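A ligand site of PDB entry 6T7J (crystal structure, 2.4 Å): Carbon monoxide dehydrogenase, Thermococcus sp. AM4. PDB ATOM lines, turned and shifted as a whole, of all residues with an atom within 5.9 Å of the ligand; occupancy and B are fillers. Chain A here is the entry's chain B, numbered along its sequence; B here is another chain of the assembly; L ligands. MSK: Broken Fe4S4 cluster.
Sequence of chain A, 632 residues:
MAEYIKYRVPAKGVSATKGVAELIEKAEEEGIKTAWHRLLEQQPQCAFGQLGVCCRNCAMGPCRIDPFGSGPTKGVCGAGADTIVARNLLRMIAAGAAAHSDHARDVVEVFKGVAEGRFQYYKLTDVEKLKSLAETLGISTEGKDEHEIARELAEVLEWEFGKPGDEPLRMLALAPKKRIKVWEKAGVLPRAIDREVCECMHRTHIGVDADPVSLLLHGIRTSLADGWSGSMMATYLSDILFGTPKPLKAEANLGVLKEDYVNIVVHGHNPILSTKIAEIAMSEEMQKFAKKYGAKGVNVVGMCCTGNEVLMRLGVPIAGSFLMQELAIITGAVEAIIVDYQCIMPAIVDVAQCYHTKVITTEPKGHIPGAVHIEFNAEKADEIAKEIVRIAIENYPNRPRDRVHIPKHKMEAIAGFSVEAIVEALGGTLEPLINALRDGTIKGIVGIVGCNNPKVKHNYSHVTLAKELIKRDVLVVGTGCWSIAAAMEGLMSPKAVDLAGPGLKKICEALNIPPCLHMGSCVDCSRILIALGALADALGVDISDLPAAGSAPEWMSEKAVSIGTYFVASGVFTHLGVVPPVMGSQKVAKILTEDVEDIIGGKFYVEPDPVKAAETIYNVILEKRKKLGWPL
The backbone carbonyl oxygen of Gly 450 lies close to a sulfur (S5) of the ligand, 3.2 Å away. Residues that only touch the ligand: Cys 304 (3.7 Å), Phe 322 (3.6 Å) and Met 556 (3.7 Å). Hydrophobic or aromatic side chains within 4 Å of the ligand: His 269, Phe 322 and Met 556. Of the 21 residues printed, 12 come within 4 Å of the ligand.
NE2 of His 269 is bound to FE1 of the ligand (2.2 Å). SG of Cys 305 binds FE1 of the ligand, at 2.3 Å. The side-chain sulfur of Cys 343 is bound to an iron atom (FE4) of the ligand (2.3 Å). The backbone NH (N) of Cys 481 sits close to a sulfur (S5) of the ligand (3.6 Å). An iron atom (FE2) of the ligand is bound by the side-chain sulfur (SG) of Cys 481. An iron atom (FE3) of the ligand is bound by the side-chain sulfur (SG) of Cys 451 (2.4 Å). The side-chain sulfur (SG) of Cys 522 sits close to a sulfur (S5) of the ligand (3.4 Å). OG of Ser 557 sits close to S3 of the ligand (3.6 Å). The side-chain amino group (NZ) of Lys 559 lies close to a sulfur (S3) of the ligand (3.7 Å).
NZ of Lys 559 sits close to NE2 of His 269, 2.9 Å away. A ring nitrogen (ND1) of His 269 lies within hydrogen-bond range of the backbone carbonyl oxygen (O) of Gln 342 (3.3 Å). The backbone NH (N) of Cys 305 sits at hydrogen-bond distance from the backbone carbonyl oxygen (O) of Gly 268 (3.4 Å). The side-chain sulfur (SG) of Cys 343 sits close to the side-chain amino group (NZ) of Lys 559, at 3.7 Å. The backbone NH of Cys 481 lies within hydrogen-bond range of the backbone carbonyl oxygen of Gly 450, at 3.5 Å. The backbone NH (N) of Met 556 lies close to the side-chain sulfur (SG) of Cys 451 (3.4 Å). The backbone NH (N) of Phe 322 lies close to the side-chain sulfur (SG) of Cys 304, at 3.7 Å. The side-chain amide oxygen (OE1) of Gln 342 lies within hydrogen-bond range of the side-chain amino group (NZ) of Lys 559 (2.8 Å).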
ATOM      1  N   GLY A 268     -16.613 -17.299  34.034  1.00  0.00           N
ATOM      2  CA  GLY A 268     -16.343 -16.102  34.815  1.00  0.00           C
ATOM      3  C   GLY A 268     -15.202 -15.262  34.284  1.00  0.00           C
ATOM      4  O   GLY A 268     -15.143 -14.991  33.074  1.00  0.00           O
ATOM      5  N   HIS A 269     -14.274 -14.850  35.153  1.00  0.00           N
ATOM      6  CA  HIS A 269     -13.280 -13.865  34.726  1.00  0.00           C
ATOM      7  C   HIS A 269     -11.919 -13.998  35.394  1.00  0.00           C
ATOM      8  O   HIS A 269     -10.887 -13.836  34.730  1.00  0.00           O
ATOM      9  CB  HIS A 269     -13.832 -12.457  34.961  1.00  0.00           C
ATOM     10  CG  HIS A 269     -14.686 -11.956  33.843  1.00  0.00           C
ATOM     11  ND1 HIS A 269     -15.970 -12.413  33.614  1.00  0.00           N
ATOM     12  CD2 HIS A 269     -14.443 -11.050  32.864  1.00  0.00           C
ATOM     13  CE1 HIS A 269     -16.469 -11.808  32.558  1.00  0.00           C
ATOM     14  NE2 HIS A 269     -15.566 -10.979  32.080  1.00  0.00           N
ATOM     15  N   CYS A 304     -16.370 -17.840  28.406  1.00  0.00           N
ATOM     16  CA  CYS A 304     -16.167 -16.400  28.598  1.00  0.00           C
ATOM     17  C   CYS A 304     -14.703 -16.139  28.957  1.00  0.00           C
ATOM     18  O   CYS A 304     -13.807 -16.880  28.532  1.00  0.00           O
ATOM     19  CB  CYS A 304     -17.183 -15.866  29.603  1.00  0.00           C
ATOM     20  SG  CYS A 304     -18.860 -15.736  28.944  1.00  0.00           S
ATOM     21  N   CYS A 305     -14.445 -15.095  29.751  1.00  0.00           N
ATOM     22  CA  CYS A 305     -13.084 -14.574  29.842  1.00  0.00           C
ATOM     23  C   CYS A 305     -12.171 -15.461  30.691  1.00  0.00           C
ATOM     24  O   CYS A 305     -10.981 -15.573  30.387  1.00  0.00           O
ATOM     25  CB  CYS A 305     -13.117 -13.143  30.382  1.00  0.00           C
ATOM     26  SG  CYS A 305     -13.405 -11.907  29.093  1.00  0.00           S
ATOM     27  N   SER A 321     -19.241 -18.733  24.133  1.00  0.00           N
ATOM     28  CA  SER A 321     -19.197 -17.350  24.563  1.00  0.00           C
ATOM     29  C   SER A 321     -20.381 -17.060  25.497  1.00  0.00           C
ATOM     30  O   SER A 321     -21.043 -17.981  25.992  1.00  0.00           O
ATOM     31  CB  SER A 321     -19.179 -16.431  23.338  1.00  0.00           C
ATOM     32  OG  SER A 321     -20.364 -16.576  22.585  1.00  0.00           O
ATOM     33  N   PHE A 322     -20.643 -15.777  25.720  1.00  0.00           N
ATOM     34  CA  PHE A 322     -21.645 -15.299  26.678  1.00  0.00           C
ATOM     35  C   PHE A 322     -22.987 -15.996  26.518  1.00  0.00           C
ATOM     36  O   PHE A 322     -23.361 -16.831  27.350  1.00  0.00           O
ATOM     37  CB  PHE A 322     -21.798 -13.782  26.524  1.00  0.00           C
ATOM     38  CG  PHE A 322     -22.803 -13.171  27.453  1.00  0.00           C
ATOM     39  CD1 PHE A 322     -22.689 -13.333  28.824  1.00  0.00           C
ATOM     40  CD2 PHE A 322     -23.852 -12.416  26.960  1.00  0.00           C
ATOM     41  CE1 PHE A 322     -23.612 -12.772  29.681  1.00  0.00           C
ATOM     42  CE2 PHE A 322     -24.776 -11.846  27.819  1.00  0.00           C
ATOM     43  CZ  PHE A 322     -24.658 -12.027  29.184  1.00  0.00           C
ATOM     44  N   GLN A 342     -18.976 -11.692  37.269  1.00  0.00           N
ATOM     45  CA  GLN A 342     -19.073 -10.970  35.999  1.00  0.00           C
ATOM     46  C   GLN A 342     -19.649 -11.828  34.883  1.00  0.00           C
ATOM     47  O   GLN A 342     -19.073 -12.860  34.499  1.00  0.00           O
ATOM     48  CB  GLN A 342     -17.715 -10.393  35.593  1.00  0.00           C
ATOM     49  CG  GLN A 342     -17.269  -9.238  36.472  1.00  0.00           C
ATOM     50  CD  GLN A 342     -15.846  -8.799  36.172  1.00  0.00           C
ATOM     51  OE1 GLN A 342     -15.389  -8.897  35.043  1.00  0.00           O
ATOM     52  NE2 GLN A 342     -15.156  -8.309  37.200  1.00  0.00           N
ATOM     53  N   CYS A 343     -20.796 -11.399  34.346  1.00  0.00           N
ATOM     54  CA  CYS A 343     -21.485 -12.023  33.212  1.00  0.00           C
ATOM     55  C   CYS A 343     -21.900 -13.462  33.495  1.00  0.00           C
ATOM     56  O   CYS A 343     -22.042 -14.276  32.581  1.00  0.00           O
ATOM     57  CB  CYS A 343     -20.621 -11.956  31.946  1.00  0.00           C
ATOM     58  SG  CYS A 343     -20.074 -10.293  31.488  1.00  0.00           S
ATOM     59  N   GLY A 450     -15.580  -7.401  22.885  1.00  0.00           N
ATOM     60  CA  GLY A 450     -16.932  -7.161  23.349  1.00  0.00           C
ATOM     61  C   GLY A 450     -17.699  -8.427  23.653  1.00  0.00           C
ATOM     62  O   GLY A 450     -17.172  -9.543  23.580  1.00  0.00           O
ATOM     63  N   CYS A 451     -18.971  -8.236  23.958  1.00  0.00           N
ATOM     64  CA  CYS A 451     -19.868  -9.222  24.528  1.00  0.00           C
ATOM     65  C   CYS A 451     -20.696  -9.906  23.433  1.00  0.00           C
ATOM     66  O   CYS A 451     -20.361  -9.843  22.245  1.00  0.00           O
ATOM     67  CB  CYS A 451     -20.761  -8.529  25.564  1.00  0.00           C
ATOM     68  SG  CYS A 451     -19.907  -7.260  26.511  1.00  0.00           S
ATOM     69  N   ASN A 452     -21.765 -10.583  23.849  1.00  0.00           N
ATOM     70  CA  ASN A 452     -22.842 -11.004  22.968  1.00  0.00           C
ATOM     71  C   ASN A 452     -24.131 -10.315  23.425  1.00  0.00           C
ATOM     72  O   ASN A 452     -24.315 -10.056  24.618  1.00  0.00           O
ATOM     73  CB  ASN A 452     -23.042 -12.525  22.979  1.00  0.00           C
ATOM     74  CG  ASN A 452     -21.972 -13.259  22.200  1.00  0.00           C
ATOM     75  OD1 ASN A 452     -21.487 -14.292  22.639  1.00  0.00           O
ATOM     76  ND2 ASN A 452     -21.616 -12.729  21.044  1.00  0.00           N
ATOM     77  N   GLY A 480     -11.824 -11.478  24.179  1.00  0.00           N
ATOM     78  CA  GLY A 480     -13.121 -11.756  24.755  1.00  0.00           C
ATOM     79  C   GLY A 480     -14.000 -12.689  23.921  1.00  0.00           C
ATOM     80  O   GLY A 480     -13.526 -13.602  23.234  1.00  0.00           O
ATOM     81  N   CYS A 481     -15.299 -12.436  24.003  1.00  0.00           N
ATOM     82  CA  CYS A 481     -16.243 -13.281  23.294  1.00  0.00           C
ATOM     83  C   CYS A 481     -16.144 -13.111  21.783  1.00  0.00           C
ATOM     84  O   CYS A 481     -16.524 -14.030  21.044  1.00  0.00           O
ATOM     85  CB  CYS A 481     -17.667 -13.014  23.788  1.00  0.00           C
ATOM     86  SG  CYS A 481     -17.965 -13.548  25.506  1.00  0.00           S
ATOM     87  N   TRP A 482     -15.606 -11.991  21.297  1.00  0.00           N
ATOM     88  CA  TRP A 482     -15.236 -11.950  19.882  1.00  0.00           C
ATOM     89  C   TRP A 482     -14.214 -13.015  19.568  1.00  0.00           C
ATOM     90  O   TRP A 482     -14.301 -13.676  18.528  1.00  0.00           O
ATOM     91  CB  TRP A 482     -14.671 -10.593  19.457  1.00  0.00           C
ATOM     92  CG  TRP A 482     -14.115 -10.705  18.039  1.00  0.00           C
ATOM     93  CD1 TRP A 482     -14.812 -10.547  16.879  1.00  0.00           C
ATOM     94  CD2 TRP A 482     -12.784 -11.082  17.652  1.00  0.00           C
ATOM     95  NE1 TRP A 482     -13.995 -10.756  15.801  1.00  0.00           N
ATOM     96  CE2 TRP A 482     -12.752 -11.092  16.248  1.00  0.00           C
ATOM     97  CE3 TRP A 482     -11.615 -11.387  18.361  1.00  0.00           C
ATOM     98  CZ2 TRP A 482     -11.595 -11.409  15.530  1.00  0.00           C
ATOM     99  CZ3 TRP A 482     -10.473 -11.700  17.651  1.00  0.00           C
ATOM    100  CH2 TRP A 482     -10.465 -11.706  16.249  1.00  0.00           C
ATOM    101  N   SER A 521      -8.343 -12.056  27.150  1.00  0.00           N
ATOM    102  CA  SER A 521      -9.630 -11.799  27.775  1.00  0.00           C
ATOM    103  C   SER A 521      -9.952 -10.303  27.738  1.00  0.00           C
ATOM    104  O   SER A 521      -9.244  -9.507  27.116  1.00  0.00           O
ATOM    105  CB  SER A 521      -9.613 -12.332  29.215  1.00  0.00           C
ATOM    106  OG  SER A 521      -8.629 -11.671  29.994  1.00  0.00           O
ATOM    107  N   CYS A 522     -11.030  -9.922  28.428  1.00  0.00           N
ATOM    108  CA  CYS A 522     -11.504  -8.541  28.393  1.00  0.00           C
ATOM    109  C   CYS A 522     -10.490  -7.591  29.019  1.00  0.00           C
ATOM    110  O   CYS A 522     -10.312  -6.460  28.540  1.00  0.00           O
ATOM    111  CB  CYS A 522     -12.846  -8.417  29.096  1.00  0.00           C
ATOM    112  SG  CYS A 522     -14.273  -8.545  27.994  1.00  0.00           S
ATOM    113  N   MET A 556     -22.698  -5.694  25.276  1.00  0.00           N
ATOM    114  CA  MET A 556     -23.839  -5.525  26.181  1.00  0.00           C
ATOM    115  C   MET A 556     -23.464  -5.028  27.577  1.00  0.00           C
ATOM    116  O   MET A 556     -24.327  -4.442  28.242  1.00  0.00           O
ATOM    117  CB  MET A 556     -24.628  -6.835  26.329  1.00  0.00           C
ATOM    118  CG  MET A 556     -23.879  -7.954  27.055  1.00  0.00           C
ATOM    119  SD  MET A 556     -24.054  -7.930  28.862  1.00  0.00           S
ATOM    120  CE  MET A 556     -22.714  -9.016  29.334  1.00  0.00           C
ATOM    121  N   SER A 557     -22.237  -5.234  28.047  1.00  0.00           N
ATOM    122  CA  SER A 557     -21.878  -4.965  29.428  1.00  0.00           C
ATOM    123  C   SER A 557     -21.392  -3.533  29.614  1.00  0.00           C
ATOM    124  O   SER A 557     -20.959  -2.862  28.676  1.00  0.00           O
ATOM    125  CB  SER A 557     -20.800  -5.949  29.902  1.00  0.00           C
ATOM    126  OG  SER A 557     -19.533  -5.565  29.402  1.00  0.00           O
ATOM    127  N   LYS A 559     -18.765  -2.988  31.325  1.00  0.00           N
ATOM    128  CA  LYS A 559     -17.340  -3.166  31.049  1.00  0.00           C
ATOM    129  C   LYS A 559     -17.013  -2.836  29.605  1.00  0.00           C
ATOM    130  O   LYS A 559     -15.985  -2.198  29.319  1.00  0.00           O
ATOM    131  CB  LYS A 559     -16.918  -4.599  31.373  1.00  0.00           C
ATOM    132  CG  LYS A 559     -16.474  -4.805  32.804  1.00  0.00           C
ATOM    133  CD  LYS A 559     -16.161  -6.270  33.061  1.00  0.00           C
ATOM    134  CE  LYS A 559     -17.396  -7.132  32.877  1.00  0.00           C
ATOM    135  NZ  LYS A 559     -17.078  -8.582  32.827  1.00  0.00           N
ATOM    136  N   ALA A 560     -17.886  -3.241  28.669  1.00  0.00           N
ATOM    137  CA  ALA A 560     -17.664  -2.916  27.258  1.00  0.00           C
ATOM    138  C   ALA A 560     -17.724  -1.413  27.029  1.00  0.00           C
ATOM    139  O   ALA A 560     -16.992  -0.880  26.197  1.00  0.00           O
ATOM    140  CB  ALA A 560     -18.691  -3.639  26.390  1.00  0.00           C
ATOM    141  N   HIS B 205     -23.131  -4.821  38.693  1.00  0.00           N
ATOM    142  CA  HIS B 205     -22.848  -5.130  37.301  1.00  0.00           C
ATOM    143  C   HIS B 205     -23.535  -6.436  36.902  1.00  0.00           C
ATOM    144  O   HIS B 205     -23.766  -7.316  37.741  1.00  0.00           O
ATOM    145  CB  HIS B 205     -21.331  -5.239  37.103  1.00  0.00           C
ATOM    146  CG  HIS B 205     -20.903  -5.332  35.671  1.00  0.00           C
ATOM    147  ND1 HIS B 205     -21.015  -6.483  34.927  1.00  0.00           N
ATOM    148  CD2 HIS B 205     -20.346  -4.413  34.847  1.00  0.00           C
ATOM    149  CE1 HIS B 205     -20.548  -6.266  33.709  1.00  0.00           C
ATOM    150  NE2 HIS B 205     -20.137  -5.021  33.631  1.00  0.00           N
HETATM  151  S1  MSK L   1     -17.165 -12.141  29.279  1.00  0.00           S
HETATM  152  S3  MSK L   1     -17.798  -8.725  29.172  1.00  0.00           S
HETATM  153  S4  MSK L   1     -20.023 -10.885  27.707  1.00  0.00           S
HETATM  154  S5  MSK L   1     -16.778 -10.434  26.622  1.00  0.00           S
HETATM  155 FE1  MSK L   1     -15.367 -10.923  29.898  1.00  0.00          FE
HETATM  156 FE2  MSK L   1     -18.168 -11.914  27.193  1.00  0.00          FE
HETATM  157 FE3  MSK L   1     -18.706  -9.230  27.204  1.00  0.00          FE
HETATM  158 FE4  MSK L   1     -18.864 -10.650  29.506  1.00  0.00          FE
